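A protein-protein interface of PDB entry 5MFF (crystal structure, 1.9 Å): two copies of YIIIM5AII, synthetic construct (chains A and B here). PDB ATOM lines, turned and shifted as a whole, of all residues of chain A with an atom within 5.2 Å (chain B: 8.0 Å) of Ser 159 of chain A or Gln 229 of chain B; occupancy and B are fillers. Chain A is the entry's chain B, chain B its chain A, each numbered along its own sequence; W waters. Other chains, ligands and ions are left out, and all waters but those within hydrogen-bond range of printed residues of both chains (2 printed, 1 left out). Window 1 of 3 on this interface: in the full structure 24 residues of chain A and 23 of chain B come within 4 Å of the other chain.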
ATOM      1  N   ALA A 116      -4.026 -29.644  -2.078  1.00  0.00           N
ATOM      2  CA  ALA A 116      -5.256 -29.174  -2.743  1.00  0.00           C
ATOM      3  C   ALA A 116      -5.124 -27.751  -3.341  1.00  0.00           C
ATOM      4  O   ALA A 116      -6.044 -27.290  -4.012  1.00  0.00           O
ATOM      5  CB  ALA A 116      -6.437 -29.245  -1.780  1.00  0.00           C
ATOM      6  N   SER A 117      -3.986 -27.066  -3.125  1.00  0.00           N
ATOM      7  CA  SER A 117      -3.763 -25.750  -3.730  1.00  0.00           C
ATOM      8  C   SER A 117      -3.121 -25.900  -5.137  1.00  0.00           C
ATOM      9  O   SER A 117      -2.900 -24.904  -5.825  1.00  0.00           O
ATOM     10  CB  SER A 117      -2.944 -24.842  -2.818  1.00  0.00           C
ATOM     11  OG  SER A 117      -1.549 -25.086  -2.936  1.00  0.00           O
ATOM     12  N   GLY A 118      -2.867 -27.146  -5.552  1.00  0.00           N
ATOM     13  CA  GLY A 118      -2.310 -27.458  -6.866  1.00  0.00           C
ATOM     14  C   GLY A 118      -3.387 -27.476  -7.935  1.00  0.00           C
ATOM     15  O   GLY A 118      -4.489 -26.946  -7.731  1.00  0.00           O
ATOM     16  N   GLY A 119      -3.074 -28.105  -9.066  1.00  0.00           N
ATOM     17  CA  GLY A 119      -4.002 -28.248 -10.186  1.00  0.00           C
ATOM     18  C   GLY A 119      -5.134 -29.224  -9.914  1.00  0.00           C
ATOM     19  O   GLY A 119      -5.186 -29.852  -8.848  1.00  0.00           O
ATOM     20  N   ASN A 120      -6.032 -29.391 -10.895  1.00  0.00           N
ATOM     21  CA  ASN A 120      -7.202 -30.264 -10.735  1.00  0.00           C
ATOM     22  C   ASN A 120      -6.853 -31.741 -10.460  1.00  0.00           C
ATOM     23  O   ASN A 120      -7.613 -32.367  -9.714  1.00  0.00           O
ATOM     24  CB  ASN A 120      -8.206 -30.121 -11.877  1.00  0.00           C
ATOM     25  CG  ASN A 120      -9.032 -28.834 -11.848  1.00  0.00           C
ATOM     26  OD1 ASN A 120      -8.810 -27.904 -11.051  1.00  0.00           O
ATOM     27  ND2 ASN A 120      -9.994 -28.735 -12.757  1.00  0.00           N
ATOM     28  N   ILE A 123      -5.955 -31.954  -6.725  1.00  0.00           N
ATOM     29  CA  ILE A 123      -7.199 -31.928  -5.958  1.00  0.00           C
ATOM     30  C   ILE A 123      -7.869 -33.304  -6.049  1.00  0.00           C
ATOM     31  O   ILE A 123      -8.277 -33.837  -5.018  1.00  0.00           O
ATOM     32  CB  ILE A 123      -8.158 -30.795  -6.419  1.00  0.00           C
ATOM     33  CG1 ILE A 123      -7.545 -29.399  -6.135  1.00  0.00           C
ATOM     34  CG2 ILE A 123      -9.525 -30.958  -5.734  1.00  0.00           C
ATOM     35  CD1 ILE A 123      -8.261 -28.227  -6.783  1.00  0.00           C
ATOM     36  N   LEU A 154     -11.294 -27.517   2.485  1.00  0.00           N
ATOM     37  CA  LEU A 154     -12.490 -27.674   1.661  1.00  0.00           C
ATOM     38  C   LEU A 154     -12.580 -26.616   0.567  1.00  0.00           C
ATOM     39  O   LEU A 154     -12.923 -26.964  -0.562  1.00  0.00           O
ATOM     40  CB  LEU A 154     -13.758 -27.676   2.508  1.00  0.00           C
ATOM     41  CG  LEU A 154     -14.036 -28.976   3.272  1.00  0.00           C
ATOM     42  CD1 LEU A 154     -15.119 -28.756   4.305  1.00  0.00           C
ATOM     43  CD2 LEU A 154     -14.468 -30.099   2.317  1.00  0.00           C
ATOM     44  N   SER A 155     -12.280 -25.336   0.894  1.00  0.00           N
ATOM     45  CA  SER A 155     -12.333 -24.248  -0.082  1.00  0.00           C
ATOM     46  C   SER A 155     -11.299 -24.439  -1.198  1.00  0.00           C
ATOM     47  O   SER A 155     -11.606 -24.121  -2.341  1.00  0.00           O
ATOM     48  CB  SER A 155     -12.218 -22.882   0.594  1.00  0.00           C
ATOM     49  OG  SER A 155     -10.911 -22.638   1.088  1.00  0.00           O
ATOM     50  N   ASN A 156     -10.118 -25.032  -0.884  1.00  0.00           N
ATOM     51  CA  ASN A 156      -9.097 -25.364  -1.874  1.00  0.00           C
ATOM     52  C   ASN A 156      -9.612 -26.476  -2.819  1.00  0.00           C
ATOM     53  O   ASN A 156      -9.563 -26.307  -4.038  1.00  0.00           O
ATOM     54  CB  ASN A 156      -7.781 -25.748  -1.200  1.00  0.00           C
ATOM     55  CG  ASN A 156      -6.951 -24.533  -0.831  1.00  0.00           C
ATOM     56  OD1 ASN A 156      -7.245 -23.396  -1.200  1.00  0.00           O
ATOM     57  ND2 ASN A 156      -5.901 -24.741  -0.086  1.00  0.00           N
ATOM     58  N   ILE A 157     -10.187 -27.551  -2.253  1.00  0.00           N
ATOM     59  CA  ILE A 157     -10.784 -28.637  -3.036  1.00  0.00           C
ATOM     60  C   ILE A 157     -11.905 -28.108  -3.942  1.00  0.00           C
ATOM     61  O   ILE A 157     -11.932 -28.438  -5.138  1.00  0.00           O
ATOM     62  CB  ILE A 157     -11.265 -29.808  -2.138  1.00  0.00           C
ATOM     63  CG1 ILE A 157     -10.053 -30.511  -1.486  1.00  0.00           C
ATOM     64  CG2 ILE A 157     -12.091 -30.807  -2.960  1.00  0.00           C
ATOM     65  CD1 ILE A 157     -10.427 -31.333  -0.274  1.00  0.00           C
ATOM     66  N   ALA A 158     -12.779 -27.244  -3.378  1.00  0.00           N
ATOM     67  CA  ALA A 158     -13.892 -26.609  -4.096  1.00  0.00           C
ATOM     68  C   ALA A 158     -13.433 -25.520  -5.087  1.00  0.00           C
ATOM     69  O   ALA A 158     -14.252 -24.985  -5.822  1.00  0.00           O
ATOM     70  CB  ALA A 158     -14.930 -26.064  -3.116  1.00  0.00           C
ATOM     71  N   SER A 159     -12.127 -25.220  -5.146  1.00  0.00           N
ATOM     72  CA  SER A 159     -11.616 -24.255  -6.120  1.00  0.00           C
ATOM     73  C   SER A 159     -11.252 -24.983  -7.452  1.00  0.00           C
ATOM     74  O   SER A 159     -10.755 -24.346  -8.390  1.00  0.00           O
ATOM     75  CB  SER A 159     -10.421 -23.490  -5.554  1.00  0.00           C
ATOM     76  OG  SER A 159      -9.213 -24.210  -5.746  1.00  0.00           O
ATOM     77  N   GLY A 160     -11.512 -26.299  -7.515  1.00  0.00           N
ATOM     78  CA  GLY A 160     -11.218 -27.121  -8.685  1.00  0.00           C
ATOM     79  C   GLY A 160     -12.320 -27.120  -9.728  1.00  0.00           C
ATOM     80  O   GLY A 160     -13.113 -26.182  -9.792  1.00  0.00           O
ATOM     81  N   GLY A 161     -12.361 -28.171 -10.542  1.00  0.00           N
ATOM     82  CA  GLY A 161     -13.359 -28.338 -11.598  1.00  0.00           C
ATOM     83  C   GLY A 161     -14.746 -28.703 -11.085  1.00  0.00           C
ATOM     84  O   GLY A 161     -14.941 -28.893  -9.874  1.00  0.00           O
ATOM     85  N   ASN A 198     -16.878 -20.726  -3.168  1.00  0.00           N
ATOM     86  CA  ASN A 198     -16.189 -21.649  -4.083  1.00  0.00           C
ATOM     87  C   ASN A 198     -17.140 -22.719  -4.624  1.00  0.00           C
ATOM     88  O   ASN A 198     -17.113 -23.024  -5.815  1.00  0.00           O
ATOM     89  CB  ASN A 198     -14.953 -22.253  -3.435  1.00  0.00           C
ATOM     90  CG  ASN A 198     -13.759 -21.344  -3.568  1.00  0.00           C
ATOM     91  OD1 ASN A 198     -13.162 -21.225  -4.638  1.00  0.00           O
ATOM     92  ND2 ASN A 198     -13.418 -20.639  -2.505  1.00  0.00           N
ATOM     93  N   GLU B 186       3.386 -22.221 -13.756  1.00  0.00           N
ATOM     94  CA  GLU B 186       1.930 -21.999 -13.713  1.00  0.00           C
ATOM     95  C   GLU B 186       1.470 -21.111 -12.557  1.00  0.00           C
ATOM     96  O   GLU B 186       0.488 -20.389 -12.715  1.00  0.00           O
ATOM     97  CB  GLU B 186       1.146 -23.329 -13.732  1.00  0.00           C
ATOM     98  CG  GLU B 186       1.129 -23.978 -15.109  1.00  0.00           C
ATOM     99  CD  GLU B 186       0.651 -25.420 -15.190  1.00  0.00           C
ATOM    100  OE1 GLU B 186       1.046 -26.239 -14.327  1.00  0.00           O
ATOM    101  OE2 GLU B 186      -0.089 -25.738 -16.151  1.00  0.00           O
ATOM    102  N   GLN B 187       2.159 -21.166 -11.408  1.00  0.00           N
ATOM    103  CA  GLN B 187       1.826 -20.327 -10.246  1.00  0.00           C
ATOM    104  C   GLN B 187       2.126 -18.841 -10.530  1.00  0.00           C
ATOM    105  O   GLN B 187       1.284 -17.983 -10.250  1.00  0.00           O
ATOM    106  CB  GLN B 187       2.515 -20.827  -8.962  1.00  0.00           C
ATOM    107  CG  GLN B 187       2.076 -22.241  -8.518  1.00  0.00           C
ATOM    108  CD  GLN B 187       0.578 -22.395  -8.300  1.00  0.00           C
ATOM    109  OE1 GLN B 187      -0.068 -21.609  -7.587  1.00  0.00           O
ATOM    110  NE2 GLN B 187      -0.010 -23.423  -8.904  1.00  0.00           N
ATOM    111  N   LEU B 189       2.385 -17.531 -13.596  1.00  0.00           N
ATOM    112  CA  LEU B 189       1.478 -17.186 -14.695  1.00  0.00           C
ATOM    113  C   LEU B 189       0.113 -16.785 -14.132  1.00  0.00           C
ATOM    114  O   LEU B 189      -0.399 -15.705 -14.467  1.00  0.00           O
ATOM    115  CB  LEU B 189       1.393 -18.378 -15.662  1.00  0.00           C
ATOM    116  CG  LEU B 189       0.631 -18.226 -16.984  1.00  0.00           C
ATOM    117  CD1 LEU B 189       1.195 -17.110 -17.824  1.00  0.00           C
ATOM    118  CD2 LEU B 189       0.732 -19.516 -17.790  1.00  0.00           C
ATOM    119  N   GLN B 190      -0.422 -17.599 -13.192  1.00  0.00           N
ATOM    120  CA  GLN B 190      -1.687 -17.306 -12.506  1.00  0.00           C
ATOM    121  C   GLN B 190      -1.662 -15.944 -11.803  1.00  0.00           C
ATOM    122  O   GLN B 190      -2.630 -15.194 -11.912  1.00  0.00           O
ATOM    123  CB  GLN B 190      -2.033 -18.394 -11.486  1.00  0.00           C
ATOM    124  CG  GLN B 190      -3.107 -19.335 -11.995  1.00  0.00           C
ATOM    125  CD  GLN B 190      -3.490 -20.366 -10.973  1.00  0.00           C
ATOM    126  OE1 GLN B 190      -2.934 -21.475 -10.936  1.00  0.00           O
ATOM    127  NE2 GLN B 190      -4.460 -20.023 -10.135  1.00  0.00           N
ATOM    128  N   LEU B 193      -1.540 -13.047 -14.418  1.00  0.00           N
ATOM    129  CA  LEU B 193      -2.882 -12.904 -14.995  1.00  0.00           C
ATOM    130  C   LEU B 193      -3.828 -12.174 -14.019  1.00  0.00           C
ATOM    131  O   LEU B 193      -4.580 -11.296 -14.445  1.00  0.00           O
ATOM    132  CB  LEU B 193      -3.472 -14.274 -15.397  1.00  0.00           C
ATOM    133  CG  LEU B 193      -2.882 -14.916 -16.635  1.00  0.00           C
ATOM    134  CD1 LEU B 193      -3.182 -16.423 -16.678  1.00  0.00           C
ATOM    135  CD2 LEU B 193      -3.407 -14.252 -17.888  1.00  0.00           C
ATOM    136  N   LEU B 222      -3.638 -18.160 -24.159  1.00  0.00           N
ATOM    137  CA  LEU B 222      -3.925 -18.860 -22.905  1.00  0.00           C
ATOM    138  C   LEU B 222      -5.371 -19.403 -22.811  1.00  0.00           C
ATOM    139  O   LEU B 222      -5.656 -20.231 -21.938  1.00  0.00           O
ATOM    140  CB  LEU B 222      -3.556 -18.005 -21.683  1.00  0.00           C
ATOM    141  CG  LEU B 222      -2.048 -17.677 -21.539  1.00  0.00           C
ATOM    142  CD1 LEU B 222      -1.841 -16.543 -20.542  1.00  0.00           C
ATOM    143  CD2 LEU B 222      -1.210 -18.935 -21.182  1.00  0.00           C
ATOM    144  N   SER B 225      -5.260 -23.090 -23.017  1.00  0.00           N
ATOM    145  CA  SER B 225      -4.604 -23.817 -21.931  1.00  0.00           C
ATOM    146  C   SER B 225      -5.405 -25.018 -21.445  1.00  0.00           C
ATOM    147  O   SER B 225      -6.596 -24.888 -21.159  1.00  0.00           O
ATOM    148  CB  SER B 225      -4.274 -22.897 -20.755  1.00  0.00           C
ATOM    149  OG  SER B 225      -3.651 -23.597 -19.686  1.00  0.00           O
ATOM    150  N   PRO B 226      -4.765 -26.195 -21.292  1.00  0.00           N
ATOM    151  CA  PRO B 226      -5.488 -27.331 -20.690  1.00  0.00           C
ATOM    152  C   PRO B 226      -5.611 -27.194 -19.149  1.00  0.00           C
ATOM    153  O   PRO B 226      -6.350 -27.959 -18.514  1.00  0.00           O
ATOM    154  CB  PRO B 226      -4.663 -28.539 -21.096  1.00  0.00           C
ATOM    155  CG  PRO B 226      -3.256 -28.003 -21.272  1.00  0.00           C
ATOM    156  CD  PRO B 226      -3.351 -26.530 -21.587  1.00  0.00           C
ATOM    157  N   ASN B 227      -4.889 -26.231 -18.549  1.00  0.00           N
ATOM    158  CA  ASN B 227      -4.955 -25.944 -17.125  1.00  0.00           C
ATOM    159  C   ASN B 227      -6.147 -24.989 -16.914  1.00  0.00           C
ATOM    160  O   ASN B 227      -6.088 -23.801 -17.269  1.00  0.00           O
ATOM    161  CB  ASN B 227      -3.628 -25.336 -16.612  1.00  0.00           C
ATOM    162  CG  ASN B 227      -3.621 -25.008 -15.137  1.00  0.00           C
ATOM    163  OD1 ASN B 227      -4.629 -24.634 -14.547  1.00  0.00           O
ATOM    164  ND2 ASN B 227      -2.470 -25.087 -14.517  1.00  0.00           N
ATOM    165  N   GLU B 228      -7.243 -25.540 -16.354  1.00  0.00           N
ATOM    166  CA  GLU B 228      -8.495 -24.805 -16.123  1.00  0.00           C
ATOM    167  C   GLU B 228      -8.346 -23.557 -15.252  1.00  0.00           C
ATOM    168  O   GLU B 228      -9.055 -22.573 -15.478  1.00  0.00           O
ATOM    169  CB  GLU B 228      -9.563 -25.731 -15.560  1.00  0.00           C
ATOM    170  CG  GLU B 228     -10.168 -26.647 -16.613  1.00  0.00           C
ATOM    171  CD  GLU B 228     -11.248 -27.588 -16.110  1.00  0.00           C
ATOM    172  OE1 GLU B 228     -11.741 -27.380 -14.978  1.00  0.00           O
ATOM    173  OE2 GLU B 228     -11.618 -28.521 -16.858  1.00  0.00           O
ATOM    174  N   GLN B 229      -7.415 -23.579 -14.282  1.00  0.00           N
ATOM    175  CA  GLN B 229      -7.203 -22.405 -13.442  1.00  0.00           C
ATOM    176  C   GLN B 229      -6.544 -21.277 -14.254  1.00  0.00           C
ATOM    177  O   GLN B 229      -6.897 -20.115 -14.065  1.00  0.00           O
ATOM    178  CB  GLN B 229      -6.431 -22.762 -12.154  1.00  0.00           C
ATOM    179  CG  GLN B 229      -7.172 -23.805 -11.294  1.00  0.00           C
ATOM    180  CD  GLN B 229      -6.360 -24.369 -10.142  1.00  0.00           C
ATOM    181  OE1 GLN B 229      -5.168 -24.069  -9.965  1.00  0.00           O
ATOM    182  NE2 GLN B 229      -6.990 -25.225  -9.332  1.00  0.00           N
ATOM    183  N   ILE B 230      -5.626 -21.621 -15.178  1.00  0.00           N
ATOM    184  CA  ILE B 230      -4.992 -20.634 -16.064  1.00  0.00           C
ATOM    185  C   ILE B 230      -6.057 -20.060 -17.005  1.00  0.00           C
ATOM    186  O   ILE B 230      -6.114 -18.846 -17.210  1.00  0.00           O
ATOM    187  CB  ILE B 230      -3.776 -21.218 -16.852  1.00  0.00           C
ATOM    188  CG1 ILE B 230      -2.550 -21.495 -15.926  1.00  0.00           C
ATOM    189  CG2 ILE B 230      -3.389 -20.347 -18.079  1.00  0.00           C
ATOM    190  CD1 ILE B 230      -1.933 -20.289 -15.160  1.00  0.00           C
ATOM    191  N   LEU B 231      -6.885 -20.952 -17.573  1.00  0.00           N
ATOM    192  CA  LEU B 231      -7.956 -20.608 -18.507  1.00  0.00           C
ATOM    193  C   LEU B 231      -8.937 -19.603 -17.886  1.00  0.00           C
ATOM    194  O   LEU B 231      -9.247 -18.589 -18.519  1.00  0.00           O
ATOM    195  CB  LEU B 231      -8.654 -21.899 -18.977  1.00  0.00           C
ATOM    196  CG  LEU B 231      -9.896 -21.813 -19.893  1.00  0.00           C
ATOM    197  CD1 LEU B 231      -9.648 -20.961 -21.114  1.00  0.00           C
ATOM    198  CD2 LEU B 231     -10.300 -23.203 -20.346  1.00  0.00           C
ATOM    199  N   GLN B 232      -9.394 -19.873 -16.658  1.00  0.00           N
ATOM    200  CA  GLN B 232     -10.318 -19.006 -15.928  1.00  0.00           C
ATOM    201  C   GLN B 232      -9.738 -17.584 -15.732  1.00  0.00           C
ATOM    202  O   GLN B 232     -10.449 -16.604 -15.941  1.00  0.00           O
ATOM    203  CB  GLN B 232     -10.686 -19.637 -14.573  1.00  0.00           C
ATOM    204  CG  GLN B 232     -11.441 -18.710 -13.629  1.00  0.00           C
ATOM    205  CD  GLN B 232     -11.994 -19.463 -12.441  1.00  0.00           C
ATOM    206  OE1 GLN B 232     -11.284 -19.787 -11.471  1.00  0.00           O
ATOM    207  NE2 GLN B 232     -13.273 -19.791 -12.515  1.00  0.00           N
ATOM    208  N   GLU B 233      -8.453 -17.503 -15.337  1.00  0.00           N
ATOM    209  CA  GLU B 233      -7.687 -16.267 -15.079  1.00  0.00           C
ATOM    210  C   GLU B 233      -7.608 -15.431 -16.377  1.00  0.00           C
ATOM    211  O   GLU B 233      -7.842 -14.223 -16.351  1.00  0.00           O
ATOM    212  CB  GLU B 233      -6.274 -16.671 -14.622  1.00  0.00           C
ATOM    213  CG  GLU B 233      -5.762 -16.052 -13.339  1.00  0.00           C
ATOM    214  CD  GLU B 233      -6.621 -16.197 -12.104  1.00  0.00           C
ATOM    215  OE1 GLU B 233      -7.040 -15.147 -11.567  1.00  0.00           O
ATOM    216  OE2 GLU B 233      -6.850 -17.343 -11.655  1.00  0.00           O
ATOM    217  N   ALA B 234      -7.300 -16.091 -17.508  1.00  0.00           N
ATOM    218  CA  ALA B 234      -7.232 -15.447 -18.825  1.00  0.00           C
ATOM    219  C   ALA B 234      -8.614 -14.963 -19.278  1.00  0.00           C
ATOM    220  O   ALA B 234      -8.727 -13.831 -19.755  1.00  0.00           O
ATOM    221  CB  ALA B 234      -6.617 -16.387 -19.854  1.00  0.00           C
ATOM    222  N   LEU B 235      -9.668 -15.796 -19.074  1.00  0.00           N
ATOM    223  CA  LEU B 235     -11.071 -15.460 -19.373  1.00  0.00           C
ATOM    224  C   LEU B 235     -11.540 -14.218 -18.613  1.00  0.00           C
ATOM    225  O   LEU B 235     -12.226 -13.366 -19.195  1.00  0.00           O
ATOM    226  CB  LEU B 235     -12.009 -16.632 -19.045  1.00  0.00           C
ATOM    227  CG  LEU B 235     -12.381 -17.524 -20.197  1.00  0.00           C
ATOM    228  CD1 LEU B 235     -13.148 -18.741 -19.707  1.00  0.00           C
ATOM    229  CD2 LEU B 235     -13.175 -16.760 -21.233  1.00  0.00           C
ATOM    230  N   ASN B 269     -16.100 -27.839 -18.306  1.00  0.00           N
ATOM    231  CA  ASN B 269     -16.351 -27.100 -17.069  1.00  0.00           C
ATOM    232  C   ASN B 269     -17.455 -26.055 -17.271  1.00  0.00           C
ATOM    233  O   ASN B 269     -17.282 -25.091 -18.016  1.00  0.00           O
ATOM    234  CB  ASN B 269     -15.065 -26.472 -16.556  1.00  0.00           C
ATOM    235  CG  ASN B 269     -15.171 -25.902 -15.165  1.00  0.00           C
ATOM    236  OD1 ASN B 269     -16.070 -25.117 -14.833  1.00  0.00           O
ATOM    237  ND2 ASN B 269     -14.200 -26.217 -14.348  1.00  0.00           N
ATOM    238  N   ILE B 272     -16.491 -22.379 -16.842  1.00  0.00           N
ATOM    239  CA  ILE B 272     -15.795 -21.869 -18.032  1.00  0.00           C
ATOM    240  C   ILE B 272     -16.843 -21.433 -19.071  1.00  0.00           C
ATOM    241  O   ILE B 272     -16.727 -20.342 -19.642  1.00  0.00           O
ATOM    242  CB  ILE B 272     -14.767 -22.901 -18.626  1.00  0.00           C
ATOM    243  CG1 ILE B 272     -13.618 -23.263 -17.611  1.00  0.00           C
ATOM    244  CG2 ILE B 272     -14.209 -22.431 -19.985  1.00  0.00           C
ATOM    245  CD1 ILE B 272     -12.694 -22.134 -17.069  1.00  0.00           C
ATOM    246  N   GLU B 275     -18.423 -18.061 -18.012  1.00  0.00           N
ATOM    247  CA  GLU B 275     -17.414 -16.996 -18.156  1.00  0.00           C
ATOM    248  C   GLU B 275     -17.185 -16.677 -19.647  1.00  0.00           C
ATOM    249  O   GLU B 275     -17.110 -15.502 -19.999  1.00  0.00           O
ATOM    250  CB  GLU B 275     -16.084 -17.382 -17.482  1.00  0.00           C
ATOM    251  CG  GLU B 275     -16.244 -17.823 -16.033  1.00  0.00           C
ATOM    252  CD  GLU B 275     -15.049 -18.439 -15.324  1.00  0.00           C
ATOM    253  OE1 GLU B 275     -14.097 -18.886 -16.000  1.00  0.00           O
ATOM    254  OE2 GLU B 275     -15.070 -18.467 -14.073  1.00  0.00           O
HETATM  255  O   HOH W   1     -11.644 -21.431  -9.074  1.00  0.00           O
HETATM  256  O   HOH W   2      -5.919 -27.346 -13.049  1.00  0.00           O
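Among the printed residues, merely in contact across the chains: Gly 161 of chain A with Asn 269 of chain B (3.6 Å), Asn 120 of chain A with Gln 229 of chain B (3.7 Å), Gly 161 of chain A with Glu 228 of chain B (3.9 Å) and Ser 159 of chain A with Gln 229 of chain B (3.98 Å).
OE1 of Glu 228 of chain B is in hydrogen-bond range of ND2 of Asn 120 of chain A. The side-chain amide nitrogen of Gln 229 of chain B lies within hydrogen-bond range of the backbone carbonyl oxygen of Gly 118 of chain A (3.4 Å).
Water W1 bridges OE1 of Gln 232 of chain B (2.9 Å) and O of Ser 159 of chain A (3.1 Å). Water W2 lies within hydrogen-bond range of N of Asn 120 of chain A (3.0 Å) and OD1 of Asn 227 of chain B (3.4 Å).
Of the 15 printed residues of chain A, 4 touch a printed residue of chain B. Among the printed residues, no Asp or Glu carboxylate lies within 4 Å of a Lys or Arg side-chain nitrogen of the other chain.
No position is printed for both chains. Of the 6 pairs that touch across the chains among the printed residues, none has its exchanged pair printed and touching as well.
Of chain B, only Gln 229 (3.98 Å) comes within 4 Å of Ser 159 of chain A. Of chain A, only Gly 118, Asn 120 and Ser 159 come within 4 Å of Gln 229 of chain B. Gly 160 of chain A touches none of the printed residues of chain B. Printed residues of chain A within 4 Å of Asn 269 of chain B: Gly 161. Printed residues of chain A within 4 Å of Glu 228 of chain B: Asn 120 and Gly 161. Printed residues of chain B within 4 Å of Gly 118 of chain A: Gln 229. Ile 230 of chain B touches none of the printed residues of chain A.
OD1 of Asn 227 of chain B sits at hydrogen-bond distance from N of Gln 229 of chain B (3.0 Å). OE1 of Glu 228 of chain B sits at hydrogen-bond distance from ND2 of Asn 269 of chain B (2.8 Å). N of Ile 272 of chain B sits at hydrogen-bond distance from OD1 of Asn 269 of chain B, 3.4 Å away. The backbone NH (N) of Gly 161 of chain A lies close to the side-chain amide nitrogen (ND2) of Asn 120 of chain A. O of Asn 156 of chain A is in hydrogen-bond range of OG of Ser 159 of chain A, 2.7 Å away.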
